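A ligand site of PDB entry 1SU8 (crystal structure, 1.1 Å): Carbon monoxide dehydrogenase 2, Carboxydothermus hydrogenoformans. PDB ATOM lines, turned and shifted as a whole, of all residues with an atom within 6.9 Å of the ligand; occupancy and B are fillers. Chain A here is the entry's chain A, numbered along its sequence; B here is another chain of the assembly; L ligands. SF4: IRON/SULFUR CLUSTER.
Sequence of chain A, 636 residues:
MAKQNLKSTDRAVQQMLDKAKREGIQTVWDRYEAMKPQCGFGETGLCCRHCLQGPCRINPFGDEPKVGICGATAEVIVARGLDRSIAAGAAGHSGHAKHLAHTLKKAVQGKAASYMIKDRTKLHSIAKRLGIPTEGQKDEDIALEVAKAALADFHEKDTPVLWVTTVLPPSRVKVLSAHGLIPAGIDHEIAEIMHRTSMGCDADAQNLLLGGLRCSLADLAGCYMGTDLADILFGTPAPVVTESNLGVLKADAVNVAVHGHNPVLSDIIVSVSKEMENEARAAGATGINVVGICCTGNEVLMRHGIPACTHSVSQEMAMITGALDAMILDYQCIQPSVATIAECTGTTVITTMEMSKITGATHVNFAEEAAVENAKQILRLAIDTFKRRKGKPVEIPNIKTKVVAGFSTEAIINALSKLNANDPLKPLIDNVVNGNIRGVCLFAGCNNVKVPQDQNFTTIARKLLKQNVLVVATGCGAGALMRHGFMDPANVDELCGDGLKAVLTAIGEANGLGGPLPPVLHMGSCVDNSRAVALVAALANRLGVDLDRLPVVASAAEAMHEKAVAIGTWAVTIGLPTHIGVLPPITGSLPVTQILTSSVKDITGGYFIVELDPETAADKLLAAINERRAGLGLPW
Residues that only touch the ligand: Gly 68 (3.9 Å), Ile 69 (3.7 Å), Ala 72 (3.96 Å) and Met 199 (3.6 Å).
Of the 29 residues printed, 12 come within 4 Å of the ligand.
The nearest printed residue that does not touch the ligand is Arg 49 (4.1 Å).
O of Gln 53 lies close to OE1 of Gln 38 of chain B.
O of Thr 197 is in hydrogen-bond range of ND1 of His 50.
The backbone carbonyl oxygen of Cys 56 sits close to the side-chain sulfur of Cys 47.
The side-chain sulfur (SD) of Met 560 of chain B sits close to the side-chain sulfur (SG) of Cys 51.
The side-chain sulfur (SG) of Cys 48 lies close to the backbone NH (N) of His 50 (3.4 Å).
N of Ile 69 lies close to SG of Cys 56 (3.5 Å).
The side-chain sulfur (SG) of Cys 70 sits close to the backbone NH (N) of Ala 72, at 3.5 Å.
The guanidinium group (NH2) of Arg 80 sits close to the side-chain sulfur (SG) of Cys 48, 3.3 Å away.
SG of Cys 48 is bound to FE2 of the ligand, at 2.3 Å.
The guanidinium group of Arg 80 lies close to a sulfur (S3) of the ligand (3.6 Å).
The backbone NH (N) of Cys 51 lies close to a sulfur (S1) of the ligand (3.6 Å).
An iron atom (FE3) of the ligand is bound by the side-chain sulfur (SG) of Cys 56 (2.3 Å).
N of Gly 54 sits close to S1 of the ligand.
S1 of the ligand sits close to N of His 50 (3.8 Å).
SG of Cys 51 is bound to FE4 of the ligand, 2.3 Å away.
A sulfur (S2) of the ligand sits close to the side-chain amide nitrogen (NE2) of Gln 53 (3.7 Å).
S2 of the ligand sits close to N of Cys 70.
FE1 of the ligand is bound by SG of Cys 70, 2.3 Å away.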
ATOM      1  N   CYS A  47      13.401 -14.119 -16.170  1.00  0.00           N
ATOM      2  CA  CYS A  47      13.609 -15.573 -16.195  1.00  0.00           C
ATOM      3  C   CYS A  47      13.320 -16.035 -14.778  1.00  0.00           C
ATOM      4  O   CYS A  47      13.717 -15.384 -13.817  1.00  0.00           O
ATOM      5  CB  CYS A  47      15.041 -15.927 -16.613  1.00  0.00           C
ATOM      6  SG  CYS A  47      15.313 -17.730 -16.517  1.00  0.00           S
ATOM      7  N   CYS A  48      12.643 -17.187 -14.732  1.00  0.00           N
ATOM      8  CA  CYS A  48      12.346 -17.839 -13.435  1.00  0.00           C
ATOM      9  C   CYS A  48      12.639 -19.340 -13.557  1.00  0.00           C
ATOM     10  O   CYS A  48      12.189 -19.973 -14.490  1.00  0.00           O
ATOM     11  CB  CYS A  48      10.881 -17.626 -13.089  1.00  0.00           C
ATOM     12  SG  CYS A  48      10.423 -18.363 -11.490  1.00  0.00           S
ATOM     13  N   ARG A  49      13.341 -19.840 -12.547  1.00  0.00           N
ATOM     14  CA  ARG A  49      13.609 -21.273 -12.399  1.00  0.00           C
ATOM     15  C   ARG A  49      13.181 -21.729 -11.008  1.00  0.00           C
ATOM     16  O   ARG A  49      13.787 -22.641 -10.464  1.00  0.00           O
ATOM     17  CB  ARG A  49      15.108 -21.525 -12.594  1.00  0.00           C
ATOM     18  CG  ARG A  49      15.520 -21.170 -13.996  1.00  0.00           C
ATOM     19  CD  ARG A  49      17.013 -21.222 -14.210  1.00  0.00           C
ATOM     20  NE  ARG A  49      17.640 -22.374 -13.745  1.00  0.00           N
ATOM     21  CZ  ARG A  49      18.801 -22.728 -13.265  1.00  0.00           C
ATOM     22  NH1 ARG A  49      19.751 -21.798 -13.200  1.00  0.00           N
ATOM     23  NH2 ARG A  49      18.966 -23.994 -12.921  1.00  0.00           N
ATOM     24  N   HIS A  50      12.156 -21.102 -10.471  1.00  0.00           N
ATOM     25  CA  HIS A  50      11.727 -21.468  -9.120  1.00  0.00           C
ATOM     26  C   HIS A  50      10.944 -22.774  -9.039  1.00  0.00           C
ATOM     27  O   HIS A  50      10.635 -23.156  -7.903  1.00  0.00           O
ATOM     28  CB  HIS A  50      10.960 -20.343  -8.430  1.00  0.00           C
ATOM     29  CG  HIS A  50      11.853 -19.114  -8.206  1.00  0.00           C
ATOM     30  ND1 HIS A  50      11.442 -18.119  -7.330  1.00  0.00           N
ATOM     31  CD2 HIS A  50      13.065 -18.745  -8.702  1.00  0.00           C
ATOM     32  CE1 HIS A  50      12.404 -17.178  -7.335  1.00  0.00           C
ATOM     33  NE2 HIS A  50      13.382 -17.526  -8.133  1.00  0.00           N
ATOM     34  N   CYS A  51      10.633 -23.422 -10.146  1.00  0.00           N
ATOM     35  CA  CYS A  51      10.090 -24.800 -10.024  1.00  0.00           C
ATOM     36  C   CYS A  51      10.509 -25.575 -11.239  1.00  0.00           C
ATOM     37  O   CYS A  51      11.044 -25.016 -12.185  1.00  0.00           O
ATOM     38  CB  CYS A  51       8.569 -24.798  -9.821  1.00  0.00           C
ATOM     39  SG  CYS A  51       7.585 -24.516 -11.326  1.00  0.00           S
ATOM     40  N   LEU A  52      10.197 -26.855 -11.197  1.00  0.00           N
ATOM     41  CA  LEU A  52      10.614 -27.771 -12.272  1.00  0.00           C
ATOM     42  C   LEU A  52       9.705 -27.757 -13.464  1.00  0.00           C
ATOM     43  O   LEU A  52       9.921 -28.519 -14.398  1.00  0.00           O
ATOM     44  CB  LEU A  52      10.714 -29.209 -11.712  1.00  0.00           C
ATOM     45  CG  LEU A  52      11.718 -29.340 -10.547  1.00  0.00           C
ATOM     46  CD1 LEU A  52      11.694 -30.812 -10.082  1.00  0.00           C
ATOM     47  CD2 LEU A  52      13.111 -28.855 -10.914  1.00  0.00           C
ATOM     48  N   GLN A  53       8.715 -26.848 -13.475  1.00  0.00           N
ATOM     49  CA  GLN A  53       8.031 -26.577 -14.716  1.00  0.00           C
ATOM     50  C   GLN A  53       8.811 -25.611 -15.589  1.00  0.00           C
ATOM     51  O   GLN A  53       8.561 -25.527 -16.801  1.00  0.00           O
ATOM     52  CB  GLN A  53       6.600 -25.983 -14.497  1.00  0.00           C
ATOM     53  CG  GLN A  53       5.764 -27.051 -13.837  1.00  0.00           C
ATOM     54  CD  GLN A  53       4.352 -26.616 -13.488  1.00  0.00           C
ATOM     55  OE1 GLN A  53       3.410 -27.396 -13.582  1.00  0.00           O
ATOM     56  NE2 GLN A  53       4.182 -25.341 -13.031  1.00  0.00           N
ATOM     57  N   GLY A  54       9.733 -24.902 -14.995  1.00  0.00           N
ATOM     58  CA  GLY A  54      10.576 -23.964 -15.686  1.00  0.00           C
ATOM     59  C   GLY A  54      11.674 -24.658 -16.480  1.00  0.00           C
ATOM     60  O   GLY A  54      11.736 -25.877 -16.561  1.00  0.00           O
ATOM     61  N   PRO A  55      12.597 -23.898 -17.047  1.00  0.00           N
ATOM     62  CA  PRO A  55      12.686 -22.445 -16.918  1.00  0.00           C
ATOM     63  C   PRO A  55      11.616 -21.717 -17.694  1.00  0.00           C
ATOM     64  O   PRO A  55      11.196 -22.128 -18.775  1.00  0.00           O
ATOM     65  CB  PRO A  55      14.075 -22.119 -17.536  1.00  0.00           C
ATOM     66  CG  PRO A  55      14.380 -23.299 -18.377  1.00  0.00           C
ATOM     67  CD  PRO A  55      13.683 -24.472 -17.872  1.00  0.00           C
ATOM     68  N   CYS A  56      11.133 -20.662 -17.052  1.00  0.00           N
ATOM     69  CA  CYS A  56      10.190 -19.741 -17.671  1.00  0.00           C
ATOM     70  C   CYS A  56      10.926 -18.476 -18.005  1.00  0.00           C
ATOM     71  O   CYS A  56      11.822 -18.039 -17.293  1.00  0.00           O
ATOM     72  CB  CYS A  56       9.027 -19.429 -16.731  1.00  0.00           C
ATOM     73  SG  CYS A  56       7.922 -20.855 -16.534  1.00  0.00           S
ATOM     74  N   ARG A  57      10.556 -17.876 -19.111  1.00  0.00           N
ATOM     75  CA  ARG A  57      11.092 -16.567 -19.483  1.00  0.00           C
ATOM     76  C   ARG A  57       9.932 -15.793 -20.073  1.00  0.00           C
ATOM     77  O   ARG A  57       8.904 -16.335 -20.430  1.00  0.00           O
ATOM     78  CB  ARG A  57      12.223 -16.750 -20.464  1.00  0.00           C
ATOM     79  CG  ARG A  57      11.727 -17.244 -21.799  1.00  0.00           C
ATOM     80  CD  ARG A  57      12.798 -17.788 -22.734  1.00  0.00           C
ATOM     81  NE  ARG A  57      12.143 -18.037 -24.056  1.00  0.00           N
ATOM     82  CZ  ARG A  57      11.344 -19.112 -24.235  1.00  0.00           C
ATOM     83  NH1 ARG A  57      10.781 -19.228 -25.461  1.00  0.00           N
ATOM     84  NH2 ARG A  57      11.044 -20.094 -23.330  1.00  0.00           N
ATOM     85  N   VAL A  67       4.049 -14.528 -19.959  1.00  0.00           N
ATOM     86  CA  VAL A  67       3.706 -14.821 -18.564  1.00  0.00           C
ATOM     87  C   VAL A  67       4.335 -16.163 -18.250  1.00  0.00           C
ATOM     88  O   VAL A  67       4.501 -17.036 -19.126  1.00  0.00           O
ATOM     89  CB  VAL A  67       2.146 -14.801 -18.423  1.00  0.00           C
ATOM     90  CG1 VAL A  67       1.466 -15.821 -19.297  1.00  0.00           C
ATOM     91  CG2 VAL A  67       1.739 -15.016 -17.000  1.00  0.00           C
ATOM     92  N   GLY A  68       4.707 -16.393 -16.993  1.00  0.00           N
ATOM     93  CA  GLY A  68       5.199 -17.689 -16.555  1.00  0.00           C
ATOM     94  C   GLY A  68       4.123 -18.764 -16.596  1.00  0.00           C
ATOM     95  O   GLY A  68       2.925 -18.511 -16.638  1.00  0.00           O
ATOM     96  N   ILE A  69       4.581 -19.990 -16.570  1.00  0.00           N
ATOM     97  CA  ILE A  69       3.663 -21.129 -16.734  1.00  0.00           C
ATOM     98  C   ILE A  69       2.623 -21.134 -15.639  1.00  0.00           C
ATOM     99  O   ILE A  69       1.452 -21.431 -15.902  1.00  0.00           O
ATOM    100  CB  ILE A  69       4.468 -22.444 -16.793  1.00  0.00           C
ATOM    101  CG1 ILE A  69       5.153 -22.540 -18.164  1.00  0.00           C
ATOM    102  CG2 ILE A  69       3.602 -23.643 -16.504  1.00  0.00           C
ATOM    103  CD1 ILE A  69       6.172 -23.628 -18.242  1.00  0.00           C
ATOM    104  N   CYS A  70       3.018 -20.823 -14.399  1.00  0.00           N
ATOM    105  CA  CYS A  70       2.038 -20.816 -13.292  1.00  0.00           C
ATOM    106  C   CYS A  70       1.186 -19.573 -13.275  1.00  0.00           C
ATOM    107  O   CYS A  70       0.293 -19.452 -12.404  1.00  0.00           O
ATOM    108  CB  CYS A  70       2.834 -20.904 -11.985  1.00  0.00           C
ATOM    109  SG  CYS A  70       3.931 -19.459 -11.782  1.00  0.00           S
ATOM    110  N   GLY A  71       1.428 -18.623 -14.193  1.00  0.00           N
ATOM    111  CA  GLY A  71       0.707 -17.345 -14.201  1.00  0.00           C
ATOM    112  C   GLY A  71       1.536 -16.189 -13.620  1.00  0.00           C
ATOM    113  O   GLY A  71       1.046 -15.064 -13.548  1.00  0.00           O
ATOM    114  N   ALA A  72       2.797 -16.450 -13.204  1.00  0.00           N
ATOM    115  CA  ALA A  72       3.629 -15.375 -12.633  1.00  0.00           C
ATOM    116  C   ALA A  72       3.885 -14.334 -13.710  1.00  0.00           C
ATOM    117  O   ALA A  72       4.393 -14.616 -14.799  1.00  0.00           O
ATOM    118  CB  ALA A  72       4.906 -15.965 -12.088  1.00  0.00           C
ATOM    119  N   THR A  73       3.540 -13.085 -13.381  1.00  0.00           N
ATOM    120  CA  THR A  73       3.760 -12.016 -14.339  1.00  0.00           C
ATOM    121  C   THR A  73       5.196 -11.550 -14.323  1.00  0.00           C
ATOM    122  O   THR A  73       6.010 -11.886 -13.458  1.00  0.00           O
ATOM    123  CB  THR A  73       2.894 -10.813 -13.963  1.00  0.00           C
ATOM    124  OG1 THR A  73       3.282 -10.403 -12.633  1.00  0.00           O
ATOM    125  CG2 THR A  73       1.392 -11.131 -13.970  1.00  0.00           C
ATOM    126  N   ILE A  77       7.933 -12.059 -11.311  1.00  0.00           N
ATOM    127  CA  ILE A  77       9.206 -12.759 -11.527  1.00  0.00           C
ATOM    128  C   ILE A  77      10.364 -11.833 -11.202  1.00  0.00           C
ATOM    129  O   ILE A  77      11.297 -12.245 -10.491  1.00  0.00           O
ATOM    130  CB  ILE A  77       9.237 -13.246 -12.988  1.00  0.00           C
ATOM    131  CG1 ILE A  77       8.269 -14.437 -13.125  1.00  0.00           C
ATOM    132  CG2 ILE A  77      10.669 -13.590 -13.426  1.00  0.00           C
ATOM    133  CD1 ILE A  77       8.159 -14.908 -14.603  1.00  0.00           C
ATOM    134  N   ARG A  80      10.569 -11.343  -7.378  1.00  0.00           N
ATOM    135  CA  ARG A  80      10.995 -12.521  -6.652  1.00  0.00           C
ATOM    136  C   ARG A  80      12.471 -12.714  -6.827  1.00  0.00           C
ATOM    137  O   ARG A  80      13.170 -13.074  -5.856  1.00  0.00           O
ATOM    138  CB  ARG A  80      10.245 -13.784  -7.140  1.00  0.00           C
ATOM    139  CG  ARG A  80       8.746 -13.712  -6.805  1.00  0.00           C
ATOM    140  CD  ARG A  80       8.025 -15.065  -6.982  1.00  0.00           C
ATOM    141  NE  ARG A  80       8.242 -15.566  -8.355  1.00  0.00           N
ATOM    142  CZ  ARG A  80       7.494 -16.560  -8.842  1.00  0.00           C
ATOM    143  NH1 ARG A  80       6.526 -17.092  -8.086  1.00  0.00           N
ATOM    144  NH2 ARG A  80       7.714 -17.021 -10.075  1.00  0.00           N
ATOM    145  N   THR A 197       8.917 -16.257  -2.101  1.00  0.00           N
ATOM    146  CA  THR A 197       9.319 -16.211  -3.505  1.00  0.00           C
ATOM    147  C   THR A 197       9.272 -17.572  -4.192  1.00  0.00           C
ATOM    148  O   THR A 197       9.538 -17.632  -5.401  1.00  0.00           O
ATOM    149  CB  THR A 197      10.729 -15.596  -3.670  1.00  0.00           C
ATOM    150  OG1 THR A 197      11.643 -16.409  -2.922  1.00  0.00           O
ATOM    151  CG2 THR A 197      10.763 -14.175  -3.194  1.00  0.00           C
ATOM    152  N   SER A 198       8.971 -18.614  -3.448  1.00  0.00           N
ATOM    153  CA  SER A 198       8.830 -19.958  -4.039  1.00  0.00           C
ATOM    154  C   SER A 198       7.525 -20.018  -4.828  1.00  0.00           C
ATOM    155  O   SER A 198       6.652 -19.115  -4.763  1.00  0.00           O
ATOM    156  CB  SER A 198       8.975 -21.016  -2.955  1.00  0.00           C
ATOM    157  OG  SER A 198       7.880 -21.122  -2.123  1.00  0.00           O
ATOM    158  N   MET A 199       7.382 -21.061  -5.618  1.00  0.00           N
ATOM    159  CA  MET A 199       6.234 -21.126  -6.540  1.00  0.00           C
ATOM    160  C   MET A 199       4.916 -21.069  -5.777  1.00  0.00           C
ATOM    161  O   MET A 199       4.691 -21.738  -4.749  1.00  0.00           O
ATOM    162  CB  MET A 199       6.422 -22.409  -7.396  1.00  0.00           C
ATOM    163  CG  MET A 199       5.262 -22.594  -8.410  1.00  0.00           C
ATOM    164  SD  MET A 199       3.801 -23.352  -7.676  1.00  0.00           S
ATOM    165  CE  MET A 199       2.876 -23.669  -9.179  1.00  0.00           C
ATOM    166  N   GLY A 200       4.006 -20.296  -6.346  1.00  0.00           N
ATOM    167  CA  GLY A 200       2.632 -20.310  -5.836  1.00  0.00           C
ATOM    168  C   GLY A 200       2.430 -19.609  -4.502  1.00  0.00           C
ATOM    169  O   GLY A 200       1.467 -19.901  -3.815  1.00  0.00           O
ATOM    170  N   VAL B  28      -2.858 -23.165 -17.530  1.00  0.00           N
ATOM    171  CA  VAL B  28      -1.441 -23.560 -17.339  1.00  0.00           C
ATOM    172  C   VAL B  28      -0.904 -24.322 -18.528  1.00  0.00           C
ATOM    173  O   VAL B  28       0.258 -24.104 -18.906  1.00  0.00           O
ATOM    174  CB  VAL B  28      -1.353 -24.390 -16.046  1.00  0.00           C
ATOM    175  CG1 VAL B  28      -2.119 -25.705 -16.114  1.00  0.00           C
ATOM    176  CG2 VAL B  28       0.100 -24.625 -15.662  1.00  0.00           C
ATOM    177  N   MET B  35       5.536 -21.318 -23.829  1.00  0.00           N
ATOM    178  CA  MET B  35       6.894 -21.236 -23.328  1.00  0.00           C
ATOM    179  C   MET B  35       7.857 -22.104 -24.108  1.00  0.00           C
ATOM    180  O   MET B  35       9.069 -22.006 -23.954  1.00  0.00           O
ATOM    181  CB  MET B  35       6.872 -21.689 -21.839  1.00  0.00           C
ATOM    182  CG  MET B  35       8.126 -21.261 -21.081  1.00  0.00           C
ATOM    183  SD  MET B  35       8.317 -19.464 -21.017  1.00  0.00           S
ATOM    184  CE  MET B  35       6.934 -19.009 -19.955  1.00  0.00           C
ATOM    185  N   GLN B  38      11.653 -24.515 -24.208  1.00  0.00           N
ATOM    186  CA  GLN B  38      12.211 -23.920 -22.980  1.00  0.00           C
ATOM    187  C   GLN B  38      13.726 -23.872 -23.083  1.00  0.00           C
ATOM    188  O   GLN B  38      14.382 -24.610 -23.797  1.00  0.00           O
ATOM    189  CB  GLN B  38      11.751 -24.727 -21.762  1.00  0.00           C
ATOM    190  CG  GLN B  38      10.264 -24.554 -21.537  1.00  0.00           C
ATOM    191  CD  GLN B  38       9.749 -25.223 -20.311  1.00  0.00           C
ATOM    192  OE1 GLN B  38       9.622 -24.598 -19.233  1.00  0.00           O
ATOM    193  NE2 GLN B  38       9.482 -26.482 -20.387  1.00  0.00           N
ATOM    194  N   PRO B 336      -0.776 -18.170  -9.554  1.00  0.00           N
ATOM    195  CA  PRO B 336      -1.325 -16.807  -9.424  1.00  0.00           C
ATOM    196  C   PRO B 336      -2.287 -16.486 -10.547  1.00  0.00           C
ATOM    197  O   PRO B 336      -3.033 -15.509 -10.447  1.00  0.00           O
ATOM    198  CB  PRO B 336      -0.084 -15.918  -9.376  1.00  0.00           C
ATOM    199  CG  PRO B 336       0.993 -16.713 -10.052  1.00  0.00           C
ATOM    200  CD  PRO B 336       0.730 -18.153  -9.648  1.00  0.00           C
ATOM    201  N   MET B 560       7.404 -30.919  -9.021  1.00  0.00           N
ATOM    202  CA  MET B 560       7.373 -29.539  -9.519  1.00  0.00           C
ATOM    203  C   MET B 560       8.070 -28.598  -8.534  1.00  0.00           C
ATOM    204  O   MET B 560       8.975 -27.869  -8.902  1.00  0.00           O
ATOM    205  CB  MET B 560       5.910 -29.124  -9.803  1.00  0.00           C
ATOM    206  CG  MET B 560       5.744 -27.698 -10.246  1.00  0.00           C
ATOM    207  SD  MET B 560       5.447 -26.479  -8.934  1.00  0.00           S
ATOM    208  CE  MET B 560       3.950 -27.128  -8.142  1.00  0.00           C
HETATM  209 FE1  SF4 L   1       6.074 -20.160 -12.200  1.00  0.00          FE
HETATM  210 FE2  SF4 L   1       8.773 -19.835 -12.079  1.00  0.00          FE
HETATM  211 FE3  SF4 L   1       7.713 -20.935 -14.261  1.00  0.00          FE
HETATM  212 FE4  SF4 L   1       7.785 -22.358 -11.950  1.00  0.00          FE
HETATM  213  S1  SF4 L   1       9.590 -21.709 -13.140  1.00  0.00           S
HETATM  214  S2  SF4 L   1       6.011 -22.141 -13.430  1.00  0.00           S
HETATM  215  S3  SF4 L   1       7.483 -20.629 -10.427  1.00  0.00           S
HETATM  216  S4  SF4 L   1       7.301 -18.779 -13.502  1.00  0.00           S
